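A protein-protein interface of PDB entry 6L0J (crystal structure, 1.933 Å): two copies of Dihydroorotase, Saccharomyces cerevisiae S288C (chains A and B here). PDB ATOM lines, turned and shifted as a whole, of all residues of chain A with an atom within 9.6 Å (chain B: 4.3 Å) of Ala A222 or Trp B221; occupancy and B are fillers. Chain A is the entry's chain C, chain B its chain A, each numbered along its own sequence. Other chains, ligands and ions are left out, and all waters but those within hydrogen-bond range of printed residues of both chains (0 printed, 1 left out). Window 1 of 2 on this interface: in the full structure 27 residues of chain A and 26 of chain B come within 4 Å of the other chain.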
ATOM      1  N   VAL A 153      -0.206 -10.735  17.516  1.00  0.00           N
ATOM      2  CA  VAL A 153      -0.416 -12.123  17.089  1.00  0.00           C
ATOM      3  C   VAL A 153      -1.729 -12.702  17.610  1.00  0.00           C
ATOM      4  O   VAL A 153      -2.253 -13.654  17.022  1.00  0.00           O
ATOM      5  CB  VAL A 153       0.761 -13.046  17.504  1.00  0.00           C
ATOM      6  CG1 VAL A 153       2.017 -12.712  16.728  1.00  0.00           C
ATOM      7  CG2 VAL A 153       1.015 -12.996  19.011  1.00  0.00           C
ATOM      8  N   LEU A 154      -2.292 -12.165  18.695  1.00  0.00           N
ATOM      9  CA  LEU A 154      -3.528 -12.768  19.183  1.00  0.00           C
ATOM     10  C   LEU A 154      -4.786 -12.190  18.530  1.00  0.00           C
ATOM     11  O   LEU A 154      -5.815 -12.869  18.503  1.00  0.00           O
ATOM     12  CB  LEU A 154      -3.635 -12.645  20.707  1.00  0.00           C
ATOM     13  CG  LEU A 154      -2.517 -13.395  21.417  1.00  0.00           C
ATOM     14  CD1 LEU A 154      -2.549 -12.980  22.865  1.00  0.00           C
ATOM     15  CD2 LEU A 154      -2.680 -14.911  21.243  1.00  0.00           C
ATOM     16  N   LEU A 216      -3.857 -27.431  20.170  1.00  0.00           N
ATOM     17  CA  LEU A 216      -2.981 -26.488  20.846  1.00  0.00           C
ATOM     18  C   LEU A 216      -3.729 -25.273  21.379  1.00  0.00           C
ATOM     19  O   LEU A 216      -4.688 -24.790  20.772  1.00  0.00           O
ATOM     20  CB  LEU A 216      -1.887 -26.013  19.892  1.00  0.00           C
ATOM     21  CG  LEU A 216      -0.949 -27.068  19.289  1.00  0.00           C
ATOM     22  CD1 LEU A 216       0.024 -26.409  18.332  1.00  0.00           C
ATOM     23  CD2 LEU A 216      -0.187 -27.838  20.354  1.00  0.00           C
ATOM     24  N   THR A 217      -3.246 -24.761  22.506  1.00  0.00           N
ATOM     25  CA  THR A 217      -3.512 -23.405  22.977  1.00  0.00           C
ATOM     26  C   THR A 217      -2.181 -22.692  23.204  1.00  0.00           C
ATOM     27  O   THR A 217      -1.093 -23.259  23.011  1.00  0.00           O
ATOM     28  CB  THR A 217      -4.351 -23.387  24.264  1.00  0.00           C
ATOM     29  OG1 THR A 217      -3.557 -23.867  25.359  1.00  0.00           O
ATOM     30  CG2 THR A 217      -5.623 -24.243  24.123  1.00  0.00           C
ATOM     31  N   ILE A 218      -2.274 -21.429  23.627  1.00  0.00           N
ATOM     32  CA  ILE A 218      -1.068 -20.640  23.846  1.00  0.00           C
ATOM     33  C   ILE A 218      -0.133 -21.314  24.848  1.00  0.00           C
ATOM     34  O   ILE A 218       1.092 -21.170  24.752  1.00  0.00           O
ATOM     35  CB  ILE A 218      -1.441 -19.209  24.287  1.00  0.00           C
ATOM     36  CG1 ILE A 218      -0.178 -18.396  24.544  1.00  0.00           C
ATOM     37  CG2 ILE A 218      -2.362 -19.226  25.504  1.00  0.00           C
ATOM     38  CD1 ILE A 218      -0.464 -16.914  24.738  1.00  0.00           C
ATOM     39  N   ASP A 219      -0.675 -22.066  25.808  1.00  0.00           N
ATOM     40  CA  ASP A 219       0.189 -22.729  26.784  1.00  0.00           C
ATOM     41  C   ASP A 219       1.128 -23.733  26.131  1.00  0.00           C
ATOM     42  O   ASP A 219       2.226 -23.978  26.646  1.00  0.00           O
ATOM     43  CB  ASP A 219      -0.637 -23.449  27.833  1.00  0.00           C
ATOM     44  CG  ASP A 219      -0.973 -22.575  28.993  1.00  0.00           C
ATOM     45  OD1 ASP A 219      -1.301 -23.135  30.045  1.00  0.00           O
ATOM     46  OD2 ASP A 219      -0.916 -21.335  28.857  1.00  0.00           O
ATOM     47  N   ASP A 220       0.713 -24.336  25.020  1.00  0.00           N
ATOM     48  CA  ASP A 220       1.498 -25.401  24.406  1.00  0.00           C
ATOM     49  C   ASP A 220       2.712 -24.874  23.658  1.00  0.00           C
ATOM     50  O   ASP A 220       3.705 -25.601  23.515  1.00  0.00           O
ATOM     51  CB  ASP A 220       0.623 -26.226  23.461  1.00  0.00           C
ATOM     52  CG  ASP A 220      -0.503 -26.908  24.182  1.00  0.00           C
ATOM     53  OD1 ASP A 220      -0.244 -27.563  25.206  1.00  0.00           O
ATOM     54  OD2 ASP A 220      -1.659 -26.750  23.753  1.00  0.00           O
ATOM     55  N   TRP A 221       2.681 -23.632  23.181  1.00  0.00           N
ATOM     56  CA  TRP A 221       3.838 -23.101  22.484  1.00  0.00           C
ATOM     57  C   TRP A 221       4.615 -22.050  23.265  1.00  0.00           C
ATOM     58  O   TRP A 221       5.669 -21.619  22.792  1.00  0.00           O
ATOM     59  CB  TRP A 221       3.435 -22.544  21.106  1.00  0.00           C
ATOM     60  CG  TRP A 221       2.429 -21.388  21.060  1.00  0.00           C
ATOM     61  CD1 TRP A 221       1.072 -21.486  20.876  1.00  0.00           C
ATOM     62  CD2 TRP A 221       2.722 -19.984  21.114  1.00  0.00           C
ATOM     63  NE1 TRP A 221       0.505 -20.238  20.843  1.00  0.00           N
ATOM     64  CE2 TRP A 221       1.493 -19.295  20.983  1.00  0.00           C
ATOM     65  CE3 TRP A 221       3.902 -19.242  21.283  1.00  0.00           C
ATOM     66  CZ2 TRP A 221       1.406 -17.898  21.024  1.00  0.00           C
ATOM     67  CZ3 TRP A 221       3.819 -17.845  21.309  1.00  0.00           C
ATOM     68  CH2 TRP A 221       2.576 -17.189  21.178  1.00  0.00           C
ATOM     69  N   ALA A 222       4.160 -21.637  24.449  1.00  0.00           N
ATOM     70  CA  ALA A 222       4.812 -20.495  25.100  1.00  0.00           C
ATOM     71  C   ALA A 222       6.321 -20.730  25.282  1.00  0.00           C
ATOM     72  O   ALA A 222       7.148 -19.879  24.922  1.00  0.00           O
ATOM     73  CB  ALA A 222       4.114 -20.169  26.426  1.00  0.00           C
ATOM     74  N   GLY A 223       6.709 -21.888  25.777  1.00  0.00           N
ATOM     75  CA  GLY A 223       8.131 -22.173  25.856  1.00  0.00           C
ATOM     76  C   GLY A 223       8.543 -23.325  24.960  1.00  0.00           C
ATOM     77  O   GLY A 223       9.563 -23.975  25.209  1.00  0.00           O
ATOM     78  N   ASN A 224       7.746 -23.600  23.921  1.00  0.00           N
ATOM     79  CA  ASN A 224       7.947 -24.762  23.054  1.00  0.00           C
ATOM     80  C   ASN A 224       7.880 -24.336  21.598  1.00  0.00           C
ATOM     81  O   ASN A 224       6.834 -24.481  20.943  1.00  0.00           O
ATOM     82  CB  ASN A 224       6.910 -25.848  23.339  1.00  0.00           C
ATOM     83  CG  ASN A 224       6.964 -26.341  24.768  1.00  0.00           C
ATOM     84  OD1 ASN A 224       8.024 -26.735  25.261  1.00  0.00           O
ATOM     85  ND2 ASN A 224       5.813 -26.332  25.445  1.00  0.00           N
ATOM     86  N   PRO A 225       8.990 -23.838  21.046  1.00  0.00           N
ATOM     87  CA  PRO A 225       8.999 -23.441  19.629  1.00  0.00           C
ATOM     88  C   PRO A 225       8.453 -24.483  18.659  1.00  0.00           C
ATOM     89  O   PRO A 225       7.969 -24.084  17.594  1.00  0.00           O
ATOM     90  CB  PRO A 225      10.485 -23.163  19.359  1.00  0.00           C
ATOM     91  CG  PRO A 225      11.022 -22.720  20.694  1.00  0.00           C
ATOM     92  CD  PRO A 225      10.277 -23.553  21.712  1.00  0.00           C
ATOM     93  N   VAL A 226       8.504 -25.786  18.971  1.00  0.00           N
ATOM     94  CA  VAL A 226       7.991 -26.758  18.003  1.00  0.00           C
ATOM     95  C   VAL A 226       6.505 -26.571  17.799  1.00  0.00           C
ATOM     96  O   VAL A 226       5.969 -26.974  16.767  1.00  0.00           O
ATOM     97  CB  VAL A 226       8.274 -28.228  18.390  1.00  0.00           C
ATOM     98  CG1 VAL A 226       9.676 -28.628  17.985  1.00  0.00           C
ATOM     99  CG2 VAL A 226       7.962 -28.507  19.850  1.00  0.00           C
ATOM    100  N   ASN A 227       5.809 -25.988  18.776  1.00  0.00           N
ATOM    101  CA  ASN A 227       4.372 -25.784  18.685  1.00  0.00           C
ATOM    102  C   ASN A 227       4.024 -24.373  18.233  1.00  0.00           C
ATOM    103  O   ASN A 227       2.844 -24.006  18.231  1.00  0.00           O
ATOM    104  CB  ASN A 227       3.702 -26.097  20.029  1.00  0.00           C
ATOM    105  CG  ASN A 227       3.751 -27.566  20.370  1.00  0.00           C
ATOM    106  OD1 ASN A 227       3.808 -28.427  19.477  1.00  0.00           O
ATOM    107  ND2 ASN A 227       3.725 -27.874  21.666  1.00  0.00           N
ATOM    108  N   PHE A 228       5.028 -23.576  17.874  1.00  0.00           N
ATOM    109  CA  PHE A 228       4.834 -22.215  17.407  1.00  0.00           C
ATOM    110  C   PHE A 228       4.560 -22.230  15.908  1.00  0.00           C
ATOM    111  O   PHE A 228       5.379 -22.722  15.134  1.00  0.00           O
ATOM    112  CB  PHE A 228       6.086 -21.386  17.702  1.00  0.00           C
ATOM    113  CG  PHE A 228       6.097 -20.041  17.042  1.00  0.00           C
ATOM    114  CD1 PHE A 228       5.166 -19.086  17.389  1.00  0.00           C
ATOM    115  CD2 PHE A 228       7.040 -19.732  16.072  1.00  0.00           C
ATOM    116  CE1 PHE A 228       5.163 -17.835  16.780  1.00  0.00           C
ATOM    117  CE2 PHE A 228       7.048 -18.488  15.462  1.00  0.00           C
ATOM    118  CZ  PHE A 228       6.106 -17.534  15.817  1.00  0.00           C
ATOM    119  N   CYS A 229       3.424 -21.692  15.490  1.00  0.00           N
ATOM    120  CA  CYS A 229       3.141 -21.544  14.079  1.00  0.00           C
ATOM    121  C   CYS A 229       2.348 -20.245  13.902  1.00  0.00           C
ATOM    122  O   CYS A 229       1.985 -19.579  14.878  1.00  0.00           O
ATOM    123  CB  CYS A 229       2.361 -22.762  13.583  1.00  0.00           C
ATOM    124  SG  CYS A 229       0.809 -22.828  14.488  1.00  0.00           S
ATOM    125  N   VAL A 232      -0.846 -18.071  15.526  1.00  0.00           N
ATOM    126  CA  VAL A 232      -0.539 -18.817  16.739  1.00  0.00           C
ATOM    127  C   VAL A 232      -1.815 -19.450  17.278  1.00  0.00           C
ATOM    128  O   VAL A 232      -2.922 -18.920  17.099  1.00  0.00           O
ATOM    129  CB  VAL A 232       0.118 -17.906  17.794  1.00  0.00           C
ATOM    130  CG1 VAL A 232       1.356 -17.220  17.223  1.00  0.00           C
ATOM    131  CG2 VAL A 232      -0.892 -16.869  18.316  1.00  0.00           C
ATOM    132  N   ALA A 233      -1.661 -20.600  17.934  1.00  0.00           N
ATOM    133  CA  ALA A 233      -2.755 -21.153  18.726  1.00  0.00           C
ATOM    134  C   ALA A 233      -3.105 -20.184  19.847  1.00  0.00           C
ATOM    135  O   ALA A 233      -2.226 -19.544  20.432  1.00  0.00           O
ATOM    136  CB  ALA A 233      -2.383 -22.519  19.317  1.00  0.00           C
ATOM    137  N   LYS A 234      -4.398 -20.074  20.146  1.00  0.00           N
ATOM    138  CA  LYS A 234      -4.878 -18.975  20.973  1.00  0.00           C
ATOM    139  C   LYS A 234      -5.501 -19.490  22.271  1.00  0.00           C
ATOM    140  O   LYS A 234      -4.931 -20.363  22.932  1.00  0.00           O
ATOM    141  CB  LYS A 234      -5.849 -18.118  20.153  1.00  0.00           C
ATOM    142  CG  LYS A 234      -5.138 -17.354  19.012  1.00  0.00           C
ATOM    143  CD  LYS A 234      -6.097 -16.791  17.960  1.00  0.00           C
ATOM    144  CE  LYS A 234      -5.406 -15.788  16.990  1.00  0.00           C
ATOM    145  NZ  LYS A 234      -4.252 -16.341  16.184  1.00  0.00           N
ATOM    146  N   ASN A 269      16.173 -21.961  17.976  1.00  0.00           N
ATOM    147  CA  ASN A 269      16.817 -20.661  17.843  1.00  0.00           C
ATOM    148  C   ASN A 269      16.469 -19.805  19.053  1.00  0.00           C
ATOM    149  O   ASN A 269      15.334 -19.838  19.531  1.00  0.00           O
ATOM    150  CB  ASN A 269      16.343 -19.929  16.577  1.00  0.00           C
ATOM    151  CG  ASN A 269      16.927 -20.512  15.305  1.00  0.00           C
ATOM    152  OD1 ASN A 269      17.724 -21.444  15.371  1.00  0.00           O
ATOM    153  ND2 ASN A 269      16.556 -19.952  14.138  1.00  0.00           N
ATOM    154  N   TYR A 270      17.420 -19.005  19.526  1.00  0.00           N
ATOM    155  CA  TYR A 270      17.050 -18.068  20.575  1.00  0.00           C
ATOM    156  C   TYR A 270      16.321 -16.844  20.030  1.00  0.00           C
ATOM    157  O   TYR A 270      15.685 -16.120  20.803  1.00  0.00           O
ATOM    158  CB  TYR A 270      18.278 -17.682  21.409  1.00  0.00           C
ATOM    159  CG  TYR A 270      19.366 -16.827  20.761  1.00  0.00           C
ATOM    160  CD1 TYR A 270      20.596 -17.376  20.436  1.00  0.00           C
ATOM    161  CD2 TYR A 270      19.181 -15.468  20.539  1.00  0.00           C
ATOM    162  CE1 TYR A 270      21.600 -16.597  19.892  1.00  0.00           C
ATOM    163  CE2 TYR A 270      20.168 -14.681  19.995  1.00  0.00           C
ATOM    164  CZ  TYR A 270      21.375 -15.246  19.674  1.00  0.00           C
ATOM    165  OH  TYR A 270      22.352 -14.460  19.128  1.00  0.00           O
ATOM    166  N   GLU A 271      16.339 -16.632  18.719  1.00  0.00           N
ATOM    167  CA  GLU A 271      15.520 -15.592  18.111  1.00  0.00           C
ATOM    168  C   GLU A 271      15.238 -15.993  16.673  1.00  0.00           C
ATOM    169  O   GLU A 271      16.004 -16.741  16.064  1.00  0.00           O
ATOM    170  CB  GLU A 271      16.196 -14.206  18.171  1.00  0.00           C
ATOM    171  CG  GLU A 271      17.595 -14.160  17.567  1.00  0.00           C
ATOM    172  CD  GLU A 271      18.244 -12.776  17.666  1.00  0.00           C
ATOM    173  OE1 GLU A 271      17.568 -11.820  18.115  1.00  0.00           O
ATOM    174  OE2 GLU A 271      19.429 -12.636  17.286  1.00  0.00           O
ATOM    175  N   GLY A 272      14.136 -15.478  16.136  1.00  0.00           N
ATOM    176  CA  GLY A 272      13.711 -15.835  14.789  1.00  0.00           C
ATOM    177  C   GLY A 272      13.414 -17.308  14.600  1.00  0.00           C
ATOM    178  O   GLY A 272      13.825 -17.904  13.594  1.00  0.00           O
ATOM    179  N   VAL A 273      12.713 -17.921  15.555  1.00  0.00           N
ATOM    180  CA  VAL A 273      12.200 -19.268  15.363  1.00  0.00           C
ATOM    181  C   VAL A 273      11.311 -19.298  14.126  1.00  0.00           C
ATOM    182  O   VAL A 273      10.440 -18.439  13.944  1.00  0.00           O
ATOM    183  CB  VAL A 273      11.435 -19.729  16.615  1.00  0.00           C
ATOM    184  CG1 VAL A 273      10.661 -21.010  16.331  1.00  0.00           C
ATOM    185  CG2 VAL A 273      12.395 -19.931  17.767  1.00  0.00           C
ATOM    186  N   THR B 217       5.893  -6.862  24.499  1.00  0.00           N
ATOM    187  CA  THR B 217       4.563  -7.439  24.400  1.00  0.00           C
ATOM    188  C   THR B 217       4.692  -8.848  23.826  1.00  0.00           C
ATOM    189  O   THR B 217       5.792  -9.299  23.470  1.00  0.00           O
ATOM    190  CB  THR B 217       3.642  -6.587  23.521  1.00  0.00           C
ATOM    191  OG1 THR B 217       4.026  -6.756  22.147  1.00  0.00           O
ATOM    192  CG2 THR B 217       3.739  -5.111  23.905  1.00  0.00           C
ATOM    193  N   ILE B 218       3.551  -9.529  23.705  1.00  0.00           N
ATOM    194  CA  ILE B 218       3.544 -10.916  23.235  1.00  0.00           C
ATOM    195  C   ILE B 218       4.190 -11.031  21.863  1.00  0.00           C
ATOM    196  O   ILE B 218       4.815 -12.052  21.547  1.00  0.00           O
ATOM    197  CB  ILE B 218       2.111 -11.490  23.231  1.00  0.00           C
ATOM    198  CG1 ILE B 218       2.101 -12.915  22.676  1.00  0.00           C
ATOM    199  CG2 ILE B 218       1.172 -10.606  22.407  1.00  0.00           C
ATOM    200  CD1 ILE B 218       0.897 -13.757  23.124  1.00  0.00           C
ATOM    201  N   ASP B 219       4.079  -9.988  21.036  1.00  0.00           N
ATOM    202  CA  ASP B 219       4.693 -10.030  19.711  1.00  0.00           C
ATOM    203  C   ASP B 219       6.210 -10.125  19.770  1.00  0.00           C
ATOM    204  O   ASP B 219       6.828 -10.604  18.816  1.00  0.00           O
ATOM    205  CB  ASP B 219       4.291  -8.798  18.899  1.00  0.00           C
ATOM    206  CG  ASP B 219       2.951  -8.969  18.202  1.00  0.00           C
ATOM    207  OD1 ASP B 219       2.752  -8.325  17.155  1.00  0.00           O
ATOM    208  OD2 ASP B 219       2.099  -9.734  18.704  1.00  0.00           O
ATOM    209  N   ASP B 220       6.826  -9.680  20.855  1.00  0.00           N
ATOM    210  CA  ASP B 220       8.279  -9.678  20.940  1.00  0.00           C
ATOM    211  C   ASP B 220       8.861 -11.027  21.332  1.00  0.00           C
ATOM    212  O   ASP B 220      10.050 -11.262  21.087  1.00  0.00           O
ATOM    213  CB  ASP B 220       8.740  -8.617  21.934  1.00  0.00           C
ATOM    214  CG  ASP B 220       8.295  -7.232  21.534  1.00  0.00           C
ATOM    215  OD1 ASP B 220       8.457  -6.891  20.347  1.00  0.00           O
ATOM    216  OD2 ASP B 220       7.757  -6.493  22.388  1.00  0.00           O
ATOM    217  N   TRP B 221       8.068 -11.916  21.942  1.00  0.00           N
ATOM    218  CA  TRP B 221       8.585 -13.217  22.335  1.00  0.00           C
ATOM    219  C   TRP B 221       7.957 -14.370  21.580  1.00  0.00           C
ATOM    220  O   TRP B 221       8.444 -15.498  21.702  1.00  0.00           O
ATOM    221  CB  TRP B 221       8.426 -13.462  23.849  1.00  0.00           C
ATOM    222  CG  TRP B 221       7.016 -13.468  24.426  1.00  0.00           C
ATOM    223  CD1 TRP B 221       6.379 -12.425  25.027  1.00  0.00           C
ATOM    224  CD2 TRP B 221       6.119 -14.581  24.514  1.00  0.00           C
ATOM    225  NE1 TRP B 221       5.129 -12.805  25.441  1.00  0.00           N
ATOM    226  CE2 TRP B 221       4.953 -14.129  25.156  1.00  0.00           C
ATOM    227  CE3 TRP B 221       6.181 -15.910  24.090  1.00  0.00           C
ATOM    228  CZ2 TRP B 221       3.860 -14.955  25.381  1.00  0.00           C
ATOM    229  CZ3 TRP B 221       5.095 -16.724  24.318  1.00  0.00           C
ATOM    230  CH2 TRP B 221       3.958 -16.247  24.962  1.00  0.00           C
ATOM    231  N   ALA B 222       6.919 -14.126  20.780  1.00  0.00           N
ATOM    232  CA  ALA B 222       6.239 -15.239  20.112  1.00  0.00           C
ATOM    233  C   ALA B 222       7.228 -16.108  19.324  1.00  0.00           C
ATOM    234  O   ALA B 222       7.273 -17.334  19.488  1.00  0.00           O
ATOM    235  CB  ALA B 222       5.126 -14.701  19.211  1.00  0.00           C
ATOM    236  N   GLY B 223       8.054 -15.488  18.500  1.00  0.00           N
ATOM    237  CA  GLY B 223       9.102 -16.256  17.851  1.00  0.00           C
ATOM    238  C   GLY B 223      10.509 -15.998  18.363  1.00  0.00           C
ATOM    239  O   GLY B 223      11.478 -16.293  17.654  1.00  0.00           O
ATOM    240  N   ASN B 224      10.657 -15.460  19.581  1.00  0.00           N
ATOM    241  CA  ASN B 224      11.966 -15.083  20.119  1.00  0.00           C
ATOM    242  C   ASN B 224      12.117 -15.586  21.553  1.00  0.00           C
ATOM    243  O   ASN B 224      11.753 -14.887  22.506  1.00  0.00           O
ATOM    244  CB  ASN B 224      12.162 -13.572  20.076  1.00  0.00           C
ATOM    245  CG  ASN B 224      12.119 -13.010  18.662  1.00  0.00           C
ATOM    246  OD1 ASN B 224      12.759 -13.534  17.752  1.00  0.00           O
ATOM    247  ND2 ASN B 224      11.356 -11.935  18.476  1.00  0.00           N
ATOM    248  N   ASN B 227      13.244 -13.446  24.594  1.00  0.00           N
ATOM    249  CA  ASN B 227      12.312 -12.535  25.238  1.00  0.00           C
ATOM    250  C   ASN B 227      11.239 -13.281  26.018  1.00  0.00           C
ATOM    251  O   ASN B 227      10.321 -12.650  26.549  1.00  0.00           O
ATOM    252  CB  ASN B 227      11.663 -11.612  24.193  1.00  0.00           C
ATOM    253  CG  ASN B 227      12.624 -10.570  23.646  1.00  0.00           C
ATOM    254  OD1 ASN B 227      13.551 -10.149  24.329  1.00  0.00           O
ATOM    255  ND2 ASN B 227      12.393 -10.139  22.410  1.00  0.00           N
ATOM    256  N   PHE B 228      11.324 -14.608  26.071  1.00  0.00           N
ATOM    257  CA  PHE B 228      10.359 -15.406  26.811  1.00  0.00           C
ATOM    258  C   PHE B 228      10.747 -15.433  28.290  1.00  0.00           C
ATOM    259  O   PHE B 228      11.873 -15.803  28.641  1.00  0.00           O
ATOM    260  CB  PHE B 228      10.286 -16.817  26.235  1.00  0.00           C
ATOM    261  CG  PHE B 228       9.475 -17.766  27.063  1.00  0.00           C
ATOM    262  CD1 PHE B 228       8.114 -17.562  27.245  1.00  0.00           C
ATOM    263  CD2 PHE B 228      10.075 -18.864  27.659  1.00  0.00           C
ATOM    264  CE1 PHE B 228       7.365 -18.432  28.007  1.00  0.00           C
ATOM    265  CE2 PHE B 228       9.327 -19.751  28.409  1.00  0.00           C
ATOM    266  CZ  PHE B 228       7.964 -19.527  28.589  1.00  0.00           C
ATOM    267  N   VAL B 232       4.582 -14.112  31.344  1.00  0.00           N
ATOM    268  CA  VAL B 232       4.892 -13.654  29.991  1.00  0.00           C
ATOM    269  C   VAL B 232       4.452 -12.202  29.809  1.00  0.00           C
ATOM    270  O   VAL B 232       3.524 -11.719  30.469  1.00  0.00           O
ATOM    271  CB  VAL B 232       4.245 -14.563  28.927  1.00  0.00           C
ATOM    272  CG1 VAL B 232       4.624 -16.024  29.152  1.00  0.00           C
ATOM    273  CG2 VAL B 232       2.718 -14.380  28.871  1.00  0.00           C
ATOM    274  N   ALA B 233       5.159 -11.490  28.931  1.00  0.00           N
ATOM    275  CA  ALA B 233       4.709 -10.181  28.481  1.00  0.00           C
ATOM    276  C   ALA B 233       3.403 -10.333  27.709  1.00  0.00           C
ATOM    277  O   ALA B 233       3.238 -11.255  26.898  1.00  0.00           O
ATOM    278  CB  ALA B 233       5.775  -9.514  27.597  1.00  0.00           C
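N of Val A153 sits at hydrogen-bond distance from OD2 of Asp B219.
O of Gly B223 is in hydrogen-bond range of N of Gly A272.
O of Gly B223 sits at hydrogen-bond distance from N of Val A273.
The backbone NH (N) of Gly A272 lies within hydrogen-bond range of the side-chain amide oxygen (OD1) of Asn B224 (2.9 Å).
The side-chain hydroxyl (OG1) of Thr B217 sits close to the backbone NH (N) of Asp B219 (3.4 Å).
The backbone carbonyl oxygen (O) of Asp B220 lies within hydrogen-bond range of the side-chain amide nitrogen (ND2) of Asn B224, 3.0 Å away.
O of Ala B233 is in hydrogen-bond range of NE1 of Trp B221 (2.8 Å).
NZ of Lys A234 is in hydrogen-bond range of O of Val A153 (3.5 Å).
The backbone NH (N) of Ile A218 lies within hydrogen-bond range of the backbone carbonyl oxygen (O) of Lys A234 (2.9 Å).
The side-chain amide nitrogen (ND2) of Asn A269 sits at hydrogen-bond distance from the backbone carbonyl oxygen (O) of Gly A272 (3.5 Å).
Among the printed residues, merely in contact across the chains: Ala A222 with Phe B228 (3.4 Å), Phe A228 with Ala B222 (3.5 Å), Trp A221 with Trp B221 (3.5 Å), Glu A271 with Asn B224 (3.5 Å), Leu A154 with Ile B218 (3.5 Å), Tyr A270 with Asn B224 (3.7 Å), Gly A223 with Phe B228 (3.7 Å), Trp A221 with Ala B222 (3.8 Å), Ile A218 with Ile B218 (3.8 Å), Ala A222 with Trp B221 (3.8 Å), Val A153 with Ile B218 (3.8 Å), Phe A228 with Gly B223 (3.8 Å) and Glu A271 with Gly B223 (3.9 Å).
Ala A222 touches two residues of chain B.
Of chain A, only Trp A221 (3.5 Å) and Ala A222 (3.8 Å) come within 4 Å of Trp B221.
Of chain A, only Trp A221 and Phe A228 come within 4 Å of Ala B222.
Gly B223 touches just these residues of chain A: Phe A228, Glu A271, Gly A272 and Val A273.
No residue of chain A comes within 4 Å of Ala B233.
Of the printed residues of chain A, Asp B219 touches Val A153.
Of the printed residues of chain B, Tyr A270 touches Asn B224 (3.7 Å).
Printed residues of chain B within 4 Å of Val A273: Gly B223 (2.9 Å).
Printed residues of chain B within 4 Å of Leu A154: Ile B218.
Of the printed residues of chain B, Glu A271 touches Gly B223 (3.9 Å) and Asn B224 (3.5 Å).
Val B232 touches none of the printed residues of chain A.
The nearest printed residue of chain B that does not touch Ala A222 is Val B232 (5.0 Å).
The nearest residue of chain A that does not touch Trp B221 is Ile A218 (4.5 Å).
The nearest printed residue of chain A that does not touch Asn B224 is Val A273 (4.9 Å).
Of the 12 printed residues of chain B, 7 touch a printed residue of chain A.
Printed residues of chain B that touch a printed residue of chain A: Ile B218, Asp B219, Trp B221, Ala B222, Gly B223, Asn B224 and Phe B228.
Hydrophobic or aromatic side chains of chain B within 4 Å of the printed part of chain A: Ile B218, Trp B221, Ala B222 and Phe B228.
Printed residues of chain A that touch a printed residue of chain B: Val A153, Leu A154, Ile A218, Trp A221, Ala A222, Gly A223, Phe A228, Tyr A270, Glu A271, Gly A272 and Val A273.
Hydrophobic or aromatic side chains of chain A that line the printed part of chain B: Val A153, Leu A154, Ile A218, Trp A221, Phe A228 and Val A273.
Trp B221 touches its own counterpart, Trp A221.
Trp A221 touches Ala B222, and with the chains exchanged Ala A222 touches Trp B221.
Ala A222 touches Phe B228, and with the chains exchanged Phe A228 touches Ala B222.
Gly A223 touches Phe B228, and with the chains exchanged Phe A228 touches Gly B223.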
